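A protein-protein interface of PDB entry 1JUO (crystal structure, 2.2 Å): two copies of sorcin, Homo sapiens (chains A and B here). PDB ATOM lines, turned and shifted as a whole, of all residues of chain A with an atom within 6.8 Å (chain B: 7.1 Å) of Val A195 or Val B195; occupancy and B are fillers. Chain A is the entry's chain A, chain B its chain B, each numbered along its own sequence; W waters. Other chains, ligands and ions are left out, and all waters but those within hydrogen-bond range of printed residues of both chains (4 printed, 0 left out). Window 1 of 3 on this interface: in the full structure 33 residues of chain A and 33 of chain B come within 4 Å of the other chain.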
ATOM      1  N   ARG A 147       3.010 -29.774  -4.923  1.00  0.00           N
ATOM      2  CA  ARG A 147       1.791 -29.195  -4.368  1.00  0.00           C
ATOM      3  C   ARG A 147       1.556 -29.588  -2.912  1.00  0.00           C
ATOM      4  O   ARG A 147       1.135 -28.759  -2.108  1.00  0.00           O
ATOM      5  CB  ARG A 147       0.580 -29.613  -5.214  1.00  0.00           C
ATOM      6  CG  ARG A 147      -0.784 -29.455  -4.531  1.00  0.00           C
ATOM      7  CD  ARG A 147      -1.256 -28.003  -4.440  1.00  0.00           C
ATOM      8  NE  ARG A 147      -2.527 -27.887  -3.720  1.00  0.00           N
ATOM      9  CZ  ARG A 147      -2.659 -28.070  -2.411  1.00  0.00           C
ATOM     10  NH1 ARG A 147      -1.602 -28.377  -1.673  1.00  0.00           N
ATOM     11  NH2 ARG A 147      -3.846 -27.941  -1.832  1.00  0.00           N
ATOM     12  N   TYR A 148       1.832 -30.844  -2.573  1.00  0.00           N
ATOM     13  CA  TYR A 148       1.623 -31.322  -1.208  1.00  0.00           C
ATOM     14  C   TYR A 148       2.870 -31.469  -0.343  1.00  0.00           C
ATOM     15  O   TYR A 148       2.830 -32.139   0.688  1.00  0.00           O
ATOM     16  CB  TYR A 148       0.880 -32.657  -1.220  1.00  0.00           C
ATOM     17  CG  TYR A 148      -0.482 -32.577  -1.845  1.00  0.00           C
ATOM     18  CD1 TYR A 148      -0.683 -32.969  -3.165  1.00  0.00           C
ATOM     19  CD2 TYR A 148      -1.563 -32.064  -1.132  1.00  0.00           C
ATOM     20  CE1 TYR A 148      -1.926 -32.846  -3.767  1.00  0.00           C
ATOM     21  CE2 TYR A 148      -2.814 -31.935  -1.727  1.00  0.00           C
ATOM     22  CZ  TYR A 148      -2.984 -32.329  -3.041  1.00  0.00           C
ATOM     23  OH  TYR A 148      -4.206 -32.200  -3.638  1.00  0.00           O
ATOM     24  N   LYS A 165      -8.787 -36.393  -4.181  1.00  0.00           N
ATOM     25  CA  LYS A 165      -8.872 -35.427  -5.266  1.00  0.00           C
ATOM     26  C   LYS A 165      -8.489 -36.085  -6.587  1.00  0.00           C
ATOM     27  O   LYS A 165      -9.131 -35.838  -7.610  1.00  0.00           O
ATOM     28  CB  LYS A 165      -7.984 -34.205  -4.978  1.00  0.00           C
ATOM     29  CG  LYS A 165      -8.239 -33.065  -5.927  1.00  0.00           C
ATOM     30  CD  LYS A 165      -7.499 -31.796  -5.546  1.00  0.00           C
ATOM     31  CE  LYS A 165      -7.751 -30.710  -6.596  1.00  0.00           C
ATOM     32  NZ  LYS A 165      -7.187 -29.364  -6.266  1.00  0.00           N
ATOM     33  N   LEU A 169     -11.172 -36.340  -9.596  1.00  0.00           N
ATOM     34  CA  LEU A 169     -10.971 -35.745 -10.905  1.00  0.00           C
ATOM     35  C   LEU A 169     -10.842 -36.787 -12.007  1.00  0.00           C
ATOM     36  O   LEU A 169     -11.302 -36.558 -13.132  1.00  0.00           O
ATOM     37  CB  LEU A 169      -9.744 -34.834 -10.888  1.00  0.00           C
ATOM     38  CG  LEU A 169      -9.829 -33.634  -9.936  1.00  0.00           C
ATOM     39  CD1 LEU A 169      -8.490 -32.929  -9.893  1.00  0.00           C
ATOM     40  CD2 LEU A 169     -10.923 -32.673 -10.387  1.00  0.00           C
ATOM     41  N   SER A 172     -14.423 -38.148 -13.023  1.00  0.00           N
ATOM     42  CA  SER A 172     -15.055 -37.173 -13.903  1.00  0.00           C
ATOM     43  C   SER A 172     -14.484 -37.209 -15.319  1.00  0.00           C
ATOM     44  O   SER A 172     -15.234 -37.240 -16.292  1.00  0.00           O
ATOM     45  CB  SER A 172     -14.900 -35.761 -13.335  1.00  0.00           C
ATOM     46  OG  SER A 172     -15.643 -35.611 -12.147  1.00  0.00           O
ATOM     47  N   PHE A 186     -13.339 -30.100 -22.968  1.00  0.00           N
ATOM     48  CA  PHE A 186     -14.076 -29.495 -21.877  1.00  0.00           C
ATOM     49  C   PHE A 186     -14.623 -28.120 -22.194  1.00  0.00           C
ATOM     50  O   PHE A 186     -13.862 -27.222 -22.553  1.00  0.00           O
ATOM     51  CB  PHE A 186     -13.162 -29.365 -20.666  1.00  0.00           C
ATOM     52  CG  PHE A 186     -13.326 -30.448 -19.652  1.00  0.00           C
ATOM     53  CD1 PHE A 186     -14.465 -30.503 -18.854  1.00  0.00           C
ATOM     54  CD2 PHE A 186     -12.321 -31.391 -19.457  1.00  0.00           C
ATOM     55  CE1 PHE A 186     -14.599 -31.476 -17.875  1.00  0.00           C
ATOM     56  CE2 PHE A 186     -12.449 -32.373 -18.472  1.00  0.00           C
ATOM     57  CZ  PHE A 186     -13.590 -32.413 -17.682  1.00  0.00           C
ATOM     58  N   ASP A 190     -18.662 -26.470 -18.009  1.00  0.00           N
ATOM     59  CA  ASP A 190     -18.543 -27.838 -17.502  1.00  0.00           C
ATOM     60  C   ASP A 190     -17.252 -28.009 -16.707  1.00  0.00           C
ATOM     61  O   ASP A 190     -17.249 -28.573 -15.615  1.00  0.00           O
ATOM     62  CB  ASP A 190     -18.587 -28.825 -18.672  1.00  0.00           C
ATOM     63  CG  ASP A 190     -18.570 -30.266 -18.221  1.00  0.00           C
ATOM     64  OD1 ASP A 190     -19.326 -30.604 -17.290  1.00  0.00           O
ATOM     65  OD2 ASP A 190     -17.806 -31.065 -18.804  1.00  0.00           O
ATOM     66  N   PHE A 191     -16.155 -27.511 -17.261  1.00  0.00           N
ATOM     67  CA  PHE A 191     -14.860 -27.589 -16.599  1.00  0.00           C
ATOM     68  C   PHE A 191     -14.914 -26.922 -15.230  1.00  0.00           C
ATOM     69  O   PHE A 191     -14.387 -27.441 -14.249  1.00  0.00           O
ATOM     70  CB  PHE A 191     -13.801 -26.918 -17.472  1.00  0.00           C
ATOM     71  CG  PHE A 191     -12.466 -26.741 -16.799  1.00  0.00           C
ATOM     72  CD1 PHE A 191     -12.164 -25.562 -16.123  1.00  0.00           C
ATOM     73  CD2 PHE A 191     -11.488 -27.727 -16.893  1.00  0.00           C
ATOM     74  CE1 PHE A 191     -10.912 -25.365 -15.557  1.00  0.00           C
ATOM     75  CE2 PHE A 191     -10.243 -27.540 -16.333  1.00  0.00           C
ATOM     76  CZ  PHE A 191      -9.948 -26.356 -15.664  1.00  0.00           C
ATOM     77  N   ILE A 192     -15.560 -25.768 -15.162  1.00  0.00           N
ATOM     78  CA  ILE A 192     -15.655 -25.054 -13.898  1.00  0.00           C
ATOM     79  C   ILE A 192     -16.473 -25.765 -12.835  1.00  0.00           C
ATOM     80  O   ILE A 192     -16.016 -25.923 -11.710  1.00  0.00           O
ATOM     81  CB  ILE A 192     -16.243 -23.633 -14.088  1.00  0.00           C
ATOM     82  CG1 ILE A 192     -15.208 -22.724 -14.745  1.00  0.00           C
ATOM     83  CG2 ILE A 192     -16.624 -23.040 -12.736  1.00  0.00           C
ATOM     84  CD1 ILE A 192     -13.947 -22.561 -13.927  1.00  0.00           C
ATOM     85  N   GLN A 193     -17.684 -26.190 -13.179  1.00  0.00           N
ATOM     86  CA  GLN A 193     -18.539 -26.847 -12.198  1.00  0.00           C
ATOM     87  C   GLN A 193     -17.945 -28.171 -11.761  1.00  0.00           C
ATOM     88  O   GLN A 193     -18.188 -28.652 -10.658  1.00  0.00           O
ATOM     89  CB  GLN A 193     -19.952 -27.055 -12.768  1.00  0.00           C
ATOM     90  CG  GLN A 193     -20.069 -28.086 -13.875  1.00  0.00           C
ATOM     91  CD  GLN A 193     -20.104 -29.501 -13.346  1.00  0.00           C
ATOM     92  OE1 GLN A 193     -19.948 -30.457 -14.105  1.00  0.00           O
ATOM     93  NE2 GLN A 193     -20.321 -29.647 -12.039  1.00  0.00           N
ATOM     94  N   CYS A 194     -17.146 -28.753 -12.637  1.00  0.00           N
ATOM     95  CA  CYS A 194     -16.527 -30.024 -12.364  1.00  0.00           C
ATOM     96  C   CYS A 194     -15.396 -29.929 -11.361  1.00  0.00           C
ATOM     97  O   CYS A 194     -15.409 -30.614 -10.341  1.00  0.00           O
ATOM     98  CB  CYS A 194     -16.005 -30.625 -13.670  1.00  0.00           C
ATOM     99  SG  CYS A 194     -15.161 -32.206 -13.481  1.00  0.00           S
ATOM    100  N   VAL A 195     -14.413 -29.083 -11.641  1.00  0.00           N
ATOM    101  CA  VAL A 195     -13.260 -28.969 -10.751  1.00  0.00           C
ATOM    102  C   VAL A 195     -13.491 -28.143  -9.474  1.00  0.00           C
ATOM    103  O   VAL A 195     -12.807 -28.350  -8.469  1.00  0.00           O
ATOM    104  CB  VAL A 195     -12.022 -28.432 -11.533  1.00  0.00           C
ATOM    105  CG1 VAL A 195     -11.950 -29.108 -12.897  1.00  0.00           C
ATOM    106  CG2 VAL A 195     -12.091 -26.929 -11.700  1.00  0.00           C
ATOM    107  N   MET A 196     -14.455 -27.223  -9.497  1.00  0.00           N
ATOM    108  CA  MET A 196     -14.739 -26.420  -8.311  1.00  0.00           C
ATOM    109  C   MET A 196     -15.372 -27.265  -7.206  1.00  0.00           C
ATOM    110  O   MET A 196     -15.354 -26.879  -6.044  1.00  0.00           O
ATOM    111  CB  MET A 196     -15.660 -25.244  -8.648  1.00  0.00           C
ATOM    112  CG  MET A 196     -14.976 -24.104  -9.394  1.00  0.00           C
ATOM    113  SD  MET A 196     -13.597 -23.369  -8.477  1.00  0.00           S
ATOM    114  CE  MET A 196     -14.470 -22.278  -7.373  1.00  0.00           C
ATOM    115  N   SER A 197     -15.939 -28.418  -7.556  1.00  0.00           N
ATOM    116  CA  SER A 197     -16.541 -29.278  -6.533  1.00  0.00           C
ATOM    117  C   SER A 197     -15.438 -29.991  -5.779  1.00  0.00           C
ATOM    118  O   SER A 197     -15.559 -30.253  -4.583  1.00  0.00           O
ATOM    119  CB  SER A 197     -17.453 -30.338  -7.161  1.00  0.00           C
ATOM    120  OG  SER A 197     -18.470 -29.724  -7.962  1.00  0.00           O
ATOM    121  N   VAL A 198     -14.356 -30.316  -6.470  1.00  0.00           N
ATOM    122  CA  VAL A 198     -13.276 -31.018  -5.806  1.00  0.00           C
ATOM    123  C   VAL A 198     -12.206 -30.052  -5.315  1.00  0.00           C
ATOM    124  O   VAL A 198     -12.407 -29.512  -4.219  1.00  0.00           O
ATOM    125  CB  VAL A 198     -12.637 -32.046  -6.744  1.00  0.00           C
ATOM    126  CG1 VAL A 198     -11.760 -32.985  -5.940  1.00  0.00           C
ATOM    127  CG2 VAL A 198     -13.718 -32.805  -7.497  1.00  0.00           C
ATOM    128  OXT VAL A 198     -11.197 -29.833  -6.024  1.00  0.00           O
ATOM    129  N   ARG B 147     -20.066 -27.100  -2.048  1.00  0.00           N
ATOM    130  CA  ARG B 147     -18.742 -27.499  -1.593  1.00  0.00           C
ATOM    131  C   ARG B 147     -18.234 -26.561  -0.532  1.00  0.00           C
ATOM    132  O   ARG B 147     -17.504 -26.973   0.394  1.00  0.00           O
ATOM    133  CB  ARG B 147     -17.768 -27.518  -2.769  1.00  0.00           C
ATOM    134  CG  ARG B 147     -16.446 -26.852  -2.512  1.00  0.00           C
ATOM    135  CD  ARG B 147     -15.459 -27.872  -2.014  1.00  0.00           C
ATOM    136  NE  ARG B 147     -14.283 -27.246  -1.431  1.00  0.00           N
ATOM    137  CZ  ARG B 147     -13.161 -27.894  -1.161  1.00  0.00           C
ATOM    138  NH1 ARG B 147     -13.021 -29.185  -1.417  1.00  0.00           N
ATOM    139  NH2 ARG B 147     -12.154 -27.229  -0.596  1.00  0.00           N
ATOM    140  N   LYS B 165      -9.523 -19.638  -6.430  1.00  0.00           N
ATOM    141  CA  LYS B 165      -9.493 -20.817  -7.297  1.00  0.00           C
ATOM    142  C   LYS B 165     -10.111 -20.512  -8.653  1.00  0.00           C
ATOM    143  O   LYS B 165      -9.606 -20.940  -9.696  1.00  0.00           O
ATOM    144  CB  LYS B 165     -10.243 -21.981  -6.657  1.00  0.00           C
ATOM    145  CG  LYS B 165      -9.714 -22.360  -5.302  1.00  0.00           C
ATOM    146  CD  LYS B 165      -9.625 -23.856  -5.130  1.00  0.00           C
ATOM    147  CE  LYS B 165     -10.979 -24.516  -5.186  1.00  0.00           C
ATOM    148  NZ  LYS B 165     -10.823 -25.981  -4.968  1.00  0.00           N
ATOM    149  N   LEU B 169      -8.110 -21.278 -12.014  1.00  0.00           N
ATOM    150  CA  LEU B 169      -8.684 -22.208 -12.979  1.00  0.00           C
ATOM    151  C   LEU B 169      -9.116 -21.528 -14.265  1.00  0.00           C
ATOM    152  O   LEU B 169      -8.989 -22.098 -15.343  1.00  0.00           O
ATOM    153  CB  LEU B 169      -9.864 -22.955 -12.354  1.00  0.00           C
ATOM    154  CG  LEU B 169      -9.420 -23.936 -11.264  1.00  0.00           C
ATOM    155  CD1 LEU B 169     -10.590 -24.307 -10.367  1.00  0.00           C
ATOM    156  CD2 LEU B 169      -8.804 -25.171 -11.918  1.00  0.00           C
ATOM    157  N   SER B 172      -6.060 -20.844 -16.328  1.00  0.00           N
ATOM    158  CA  SER B 172      -5.582 -22.085 -16.934  1.00  0.00           C
ATOM    159  C   SER B 172      -6.405 -22.499 -18.139  1.00  0.00           C
ATOM    160  O   SER B 172      -5.863 -22.990 -19.127  1.00  0.00           O
ATOM    161  CB  SER B 172      -5.598 -23.224 -15.917  1.00  0.00           C
ATOM    162  OG  SER B 172      -4.564 -23.073 -14.972  1.00  0.00           O
ATOM    163  N   ARG B 176      -5.364 -22.094 -22.523  1.00  0.00           N
ATOM    164  CA  ARG B 176      -5.401 -23.221 -23.454  1.00  0.00           C
ATOM    165  C   ARG B 176      -6.462 -23.162 -24.558  1.00  0.00           C
ATOM    166  O   ARG B 176      -6.506 -24.046 -25.397  1.00  0.00           O
ATOM    167  CB  ARG B 176      -5.603 -24.530 -22.676  1.00  0.00           C
ATOM    168  CG  ARG B 176      -4.495 -24.931 -21.695  1.00  0.00           C
ATOM    169  CD  ARG B 176      -4.990 -26.115 -20.846  1.00  0.00           C
ATOM    170  NE  ARG B 176      -3.994 -26.736 -19.970  1.00  0.00           N
ATOM    171  CZ  ARG B 176      -3.492 -26.185 -18.868  1.00  0.00           C
ATOM    172  NH1 ARG B 176      -3.882 -24.979 -18.474  1.00  0.00           N
ATOM    173  NH2 ARG B 176      -2.592 -26.846 -18.158  1.00  0.00           N
ATOM    174  N   PHE B 186      -8.407 -31.180 -23.570  1.00  0.00           N
ATOM    175  CA  PHE B 186      -7.588 -31.542 -22.427  1.00  0.00           C
ATOM    176  C   PHE B 186      -7.041 -32.963 -22.384  1.00  0.00           C
ATOM    177  O   PHE B 186      -7.797 -33.921 -22.222  1.00  0.00           O
ATOM    178  CB  PHE B 186      -8.391 -31.319 -21.138  1.00  0.00           C
ATOM    179  CG  PHE B 186      -8.067 -30.049 -20.413  1.00  0.00           C
ATOM    180  CD1 PHE B 186      -6.786 -29.813 -19.926  1.00  0.00           C
ATOM    181  CD2 PHE B 186      -9.057 -29.115 -20.161  1.00  0.00           C
ATOM    182  CE1 PHE B 186      -6.501 -28.669 -19.191  1.00  0.00           C
ATOM    183  CE2 PHE B 186      -8.780 -27.967 -19.425  1.00  0.00           C
ATOM    184  CZ  PHE B 186      -7.499 -27.744 -18.941  1.00  0.00           C
ATOM    185  N   ASP B 190      -2.349 -33.523 -18.725  1.00  0.00           N
ATOM    186  CA  ASP B 190      -2.412 -32.065 -18.636  1.00  0.00           C
ATOM    187  C   ASP B 190      -3.586 -31.615 -17.751  1.00  0.00           C
ATOM    188  O   ASP B 190      -3.457 -30.687 -16.948  1.00  0.00           O
ATOM    189  CB  ASP B 190      -2.551 -31.472 -20.039  1.00  0.00           C
ATOM    190  CG  ASP B 190      -2.511 -29.953 -20.044  1.00  0.00           C
ATOM    191  OD1 ASP B 190      -3.402 -29.341 -20.667  1.00  0.00           O
ATOM    192  OD2 ASP B 190      -1.590 -29.370 -19.432  1.00  0.00           O
ATOM    193  N   PHE B 191      -4.733 -32.267 -17.907  1.00  0.00           N
ATOM    194  CA  PHE B 191      -5.910 -31.942 -17.101  1.00  0.00           C
ATOM    195  C   PHE B 191      -5.575 -32.130 -15.626  1.00  0.00           C
ATOM    196  O   PHE B 191      -5.977 -31.330 -14.788  1.00  0.00           O
ATOM    197  CB  PHE B 191      -7.081 -32.862 -17.483  1.00  0.00           C
ATOM    198  CG  PHE B 191      -8.272 -32.772 -16.550  1.00  0.00           C
ATOM    199  CD1 PHE B 191      -9.143 -31.687 -16.604  1.00  0.00           C
ATOM    200  CD2 PHE B 191      -8.520 -33.780 -15.625  1.00  0.00           C
ATOM    201  CE1 PHE B 191     -10.243 -31.613 -15.752  1.00  0.00           C
ATOM    202  CE2 PHE B 191      -9.617 -33.716 -14.767  1.00  0.00           C
ATOM    203  CZ  PHE B 191     -10.478 -32.632 -14.831  1.00  0.00           C
ATOM    204  N   ILE B 192      -4.835 -33.191 -15.318  1.00  0.00           N
ATOM    205  CA  ILE B 192      -4.449 -33.498 -13.939  1.00  0.00           C
ATOM    206  C   ILE B 192      -3.480 -32.497 -13.315  1.00  0.00           C
ATOM    207  O   ILE B 192      -3.698 -32.020 -12.202  1.00  0.00           O
ATOM    208  CB  ILE B 192      -3.840 -34.916 -13.831  1.00  0.00           C
ATOM    209  CG1 ILE B 192      -4.945 -35.956 -13.965  1.00  0.00           C
ATOM    210  CG2 ILE B 192      -3.176 -35.106 -12.488  1.00  0.00           C
ATOM    211  CD1 ILE B 192      -6.014 -35.817 -12.908  1.00  0.00           C
ATOM    212  N   GLN B 193      -2.400 -32.193 -14.018  1.00  0.00           N
ATOM    213  CA  GLN B 193      -1.427 -31.239 -13.507  1.00  0.00           C
ATOM    214  C   GLN B 193      -2.071 -29.874 -13.290  1.00  0.00           C
ATOM    215  O   GLN B 193      -1.779 -29.180 -12.321  1.00  0.00           O
ATOM    216  CB  GLN B 193      -0.268 -31.088 -14.485  1.00  0.00           C
ATOM    217  CG  GLN B 193       0.622 -32.289 -14.575  1.00  0.00           C
ATOM    218  CD  GLN B 193       1.793 -32.047 -15.492  1.00  0.00           C
ATOM    219  OE1 GLN B 193       2.605 -31.156 -15.256  1.00  0.00           O
ATOM    220  NE2 GLN B 193       1.884 -32.836 -16.555  1.00  0.00           N
ATOM    221  N   CYS B 194      -2.948 -29.501 -14.209  1.00  0.00           N
ATOM    222  CA  CYS B 194      -3.636 -28.223 -14.155  1.00  0.00           C
ATOM    223  C   CYS B 194      -4.506 -28.046 -12.914  1.00  0.00           C
ATOM    224  O   CYS B 194      -4.457 -27.005 -12.253  1.00  0.00           O
ATOM    225  CB  CYS B 194      -4.490 -28.069 -15.415  1.00  0.00           C
ATOM    226  SG  CYS B 194      -5.586 -26.644 -15.439  1.00  0.00           S
ATOM    227  N   VAL B 195      -5.301 -29.061 -12.591  1.00  0.00           N
ATOM    228  CA  VAL B 195      -6.202 -28.966 -11.449  1.00  0.00           C
ATOM    229  C   VAL B 195      -5.523 -29.269 -10.122  1.00  0.00           C
ATOM    230  O   VAL B 195      -5.861 -28.668  -9.101  1.00  0.00           O
ATOM    231  CB  VAL B 195      -7.429 -29.909 -11.624  1.00  0.00           C
ATOM    232  CG1 VAL B 195      -8.468 -29.618 -10.560  1.00  0.00           C
ATOM    233  CG2 VAL B 195      -8.042 -29.720 -13.002  1.00  0.00           C
ATOM    234  N   MET B 196      -4.563 -30.189 -10.133  1.00  0.00           N
ATOM    235  CA  MET B 196      -3.864 -30.544  -8.908  1.00  0.00           C
ATOM    236  C   MET B 196      -2.941 -29.435  -8.438  1.00  0.00           C
ATOM    237  O   MET B 196      -2.527 -29.426  -7.283  1.00  0.00           O
ATOM    238  CB  MET B 196      -3.054 -31.837  -9.085  1.00  0.00           C
ATOM    239  CG  MET B 196      -3.881 -33.105  -9.303  1.00  0.00           C
ATOM    240  SD  MET B 196      -5.084 -33.435  -7.992  1.00  0.00           S
ATOM    241  CE  MET B 196      -4.038 -34.018  -6.700  1.00  0.00           C
ATOM    242  N   SER B 197      -2.609 -28.488  -9.310  1.00  0.00           N
ATOM    243  CA  SER B 197      -1.714 -27.410  -8.871  1.00  0.00           C
ATOM    244  C   SER B 197      -2.407 -26.319  -8.077  1.00  0.00           C
ATOM    245  O   SER B 197      -1.757 -25.567  -7.333  1.00  0.00           O
ATOM    246  CB  SER B 197      -0.948 -26.792 -10.049  1.00  0.00           C
ATOM    247  OG  SER B 197      -1.808 -26.305 -11.068  1.00  0.00           O
ATOM    248  N   VAL B 198      -3.723 -26.213  -8.210  1.00  0.00           N
ATOM    249  CA  VAL B 198      -4.446 -25.208  -7.455  1.00  0.00           C
ATOM    250  C   VAL B 198      -4.474 -25.638  -5.989  1.00  0.00           C
ATOM    251  O   VAL B 198      -4.220 -24.790  -5.105  1.00  0.00           O
ATOM    252  CB  VAL B 198      -5.877 -25.051  -7.986  1.00  0.00           C
ATOM    253  CG1 VAL B 198      -6.647 -24.056  -7.136  1.00  0.00           C
ATOM    254  CG2 VAL B 198      -5.831 -24.579  -9.426  1.00  0.00           C
ATOM    255  OXT VAL B 198      -4.742 -26.833  -5.736  1.00  0.00           O
HETATM  256  O   HOH W   1      -9.287 -28.479  -4.134  1.00  0.00           O
HETATM  257  O   HOH W   2      -4.499 -30.114  -5.430  1.00  0.00           O
HETATM  258  O   HOH W   3      -9.500 -27.457  -7.632  1.00  0.00           O
HETATM  259  O   HOH W   4     -13.188 -27.057  -4.258  1.00  0.00           O
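Water W4 lies within hydrogen-bond range of O of Val A198 (2.6 Å), NZ of Lys B165 (2.7 Å), O of Met A196 (2.8 Å) and NE of Arg B147 (3.0 Å).
Water W2 lies within hydrogen-bond range of OH of Tyr A148 (2.8 Å), O of Met B196 (2.8 Å), NZ of Lys A165 (2.9 Å), OXT of Val B198 (3.3 Å) and NE of Arg A147 (3.4 Å).
Water W1 lies within hydrogen-bond range of OXT of Val A198 (3.0 Å), NZ of Lys B165 (3.0 Å) and NZ of Lys A165 (3.1 Å).
Water W3 lies within hydrogen-bond range of NZ of Lys A165 (3.3 Å), NZ of Lys B165 (3.3 Å) and OXT of Val A198 (3.3 Å).
OG of Ser B197 sits at hydrogen-bond distance from O of Gln B193 (3.1 Å).
The backbone carbonyl oxygen (O) of Gln A193 is in hydrogen-bond range of the side-chain hydroxyl (OG) of Ser A197, 2.9 Å away.
The side-chain hydroxyl of Ser B197 lies within hydrogen-bond range of the backbone carbonyl oxygen of Cys B194 (3.0 Å).
Val A195 touches just these residues of chain B: Leu B169 and Val B195.
Of chain A, only Lys A165, Leu A169 and Val A195 come within 4 Å of Val B195.
Printed residues of chain A within 4 Å of Met B196: Arg A147 (3.3 Å), Tyr A148 (3.6 Å), Lys A165 (3.8 Å) and Leu A169 (3.9 Å).
Of the printed residues of chain B, Ser A197 touches Arg B147 (3.5 Å).
Ser B172 touches none of the printed residues of chain A.
The nearest residue of chain B that does not touch Val A195 is Phe B191 (4.2 Å).
The chain-end carboxylate (O) of Val A198 lies within salt-bridge range of the side-chain amino group (NZ) of Lys B165 (3.9 Å).
The chain-end carboxylate (OXT) of Val B198 lies within salt-bridge range of the side-chain amino group (NZ) of Lys A165 (3.6 Å).
OXT of Val B198 is in salt-bridge range of NE of Arg A147, at 3.2 Å.
The chain-end carboxylate (O) of Val A198 is in salt-bridge range of the guanidinium group (NH1) of Arg B147.
The side-chain amino group (NZ) of Lys A165 sits at hydrogen-bond distance from the backbone carbonyl oxygen (O) of Val B195 (3.2 Å).
Among the printed residues, pairs that only touch across the chains: Arg A147 with Met B196 (3.3 Å), Arg A147 with Ser B197 (3.8 Å), Tyr A148 with Met B196 (3.6 Å), Lys A165 with Met B196 (3.8 Å), Leu A169 with Phe B191 (3.7 Å), Leu A169 with Val B195 (3.4 Å), Leu A169 with Met B196 (3.9 Å), Phe A186 with Phe B191 (3.6 Å), Phe A191 with Leu B169 (3.8 Å), Phe A191 with Phe B186 (3.4 Å), Val A195 with Leu B169 (3.3 Å), Val A195 with Val B195 (3.9 Å), Met A196 with Arg B147 (3.7 Å), Met A196 with Leu B169 (3.7 Å) and Ser A197 with Arg B147 (3.5 Å).
Arg A147 touches Met B196, and with the chains exchanged Met A196 touches Arg B147.
Arg A147 touches Val B198, and with the chains exchanged Val A198 touches Arg B147.
Lys A165 touches Val B195, but with the chains exchanged Val A195 does not touch Lys B165 (4.7 Å).
Phe A186 touches Phe B191, and with the chains exchanged Phe A191 touches Phe B186.
Positions printed for both chains: 147, 165, 169, 172, 186, 190, 191, 192, 193, 194, 195, 196, 197 and 198.
Of the 20 pairs that touch across the chains among the printed residues, 17 have their exchanged pair printed and touching as well.
Of the 15 printed residues of chain B, 9 touch a printed residue of chain A.
Printed residues of chain B that touch a printed residue of chain A: Arg B147, Lys B165, Leu B169, Phe B186, Phe B191, Val B195, Met B196, Ser B197 and Val B198.
Hydrophobic or aromatic side chains of chain B within 4 Å of the printed part of chain A: Leu B169, Phe B186, Phe B191, Val B195 and Met B196.
Along chain B the printed residues that touch a printed residue of chain A span positions 147 to 198.
Printed residues of chain A that touch a printed residue of chain B: Arg A147, Tyr A148, Lys A165, Leu A169, Phe A186, Phe A191, Val A195, Met A196, Ser A197 and Val A198.
Hydrophobic or aromatic side chains of chain A that line the printed part of chain B: Tyr A148, Leu A169, Phe A186, Phe A191, Val A195 and Met A196.
Among the printed residues, 20 pairs touch across the chains.
Among the printed residues, no Asp or Glu carboxylate lies within 4 Å of a Lys or Arg side-chain nitrogen of the other chain.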
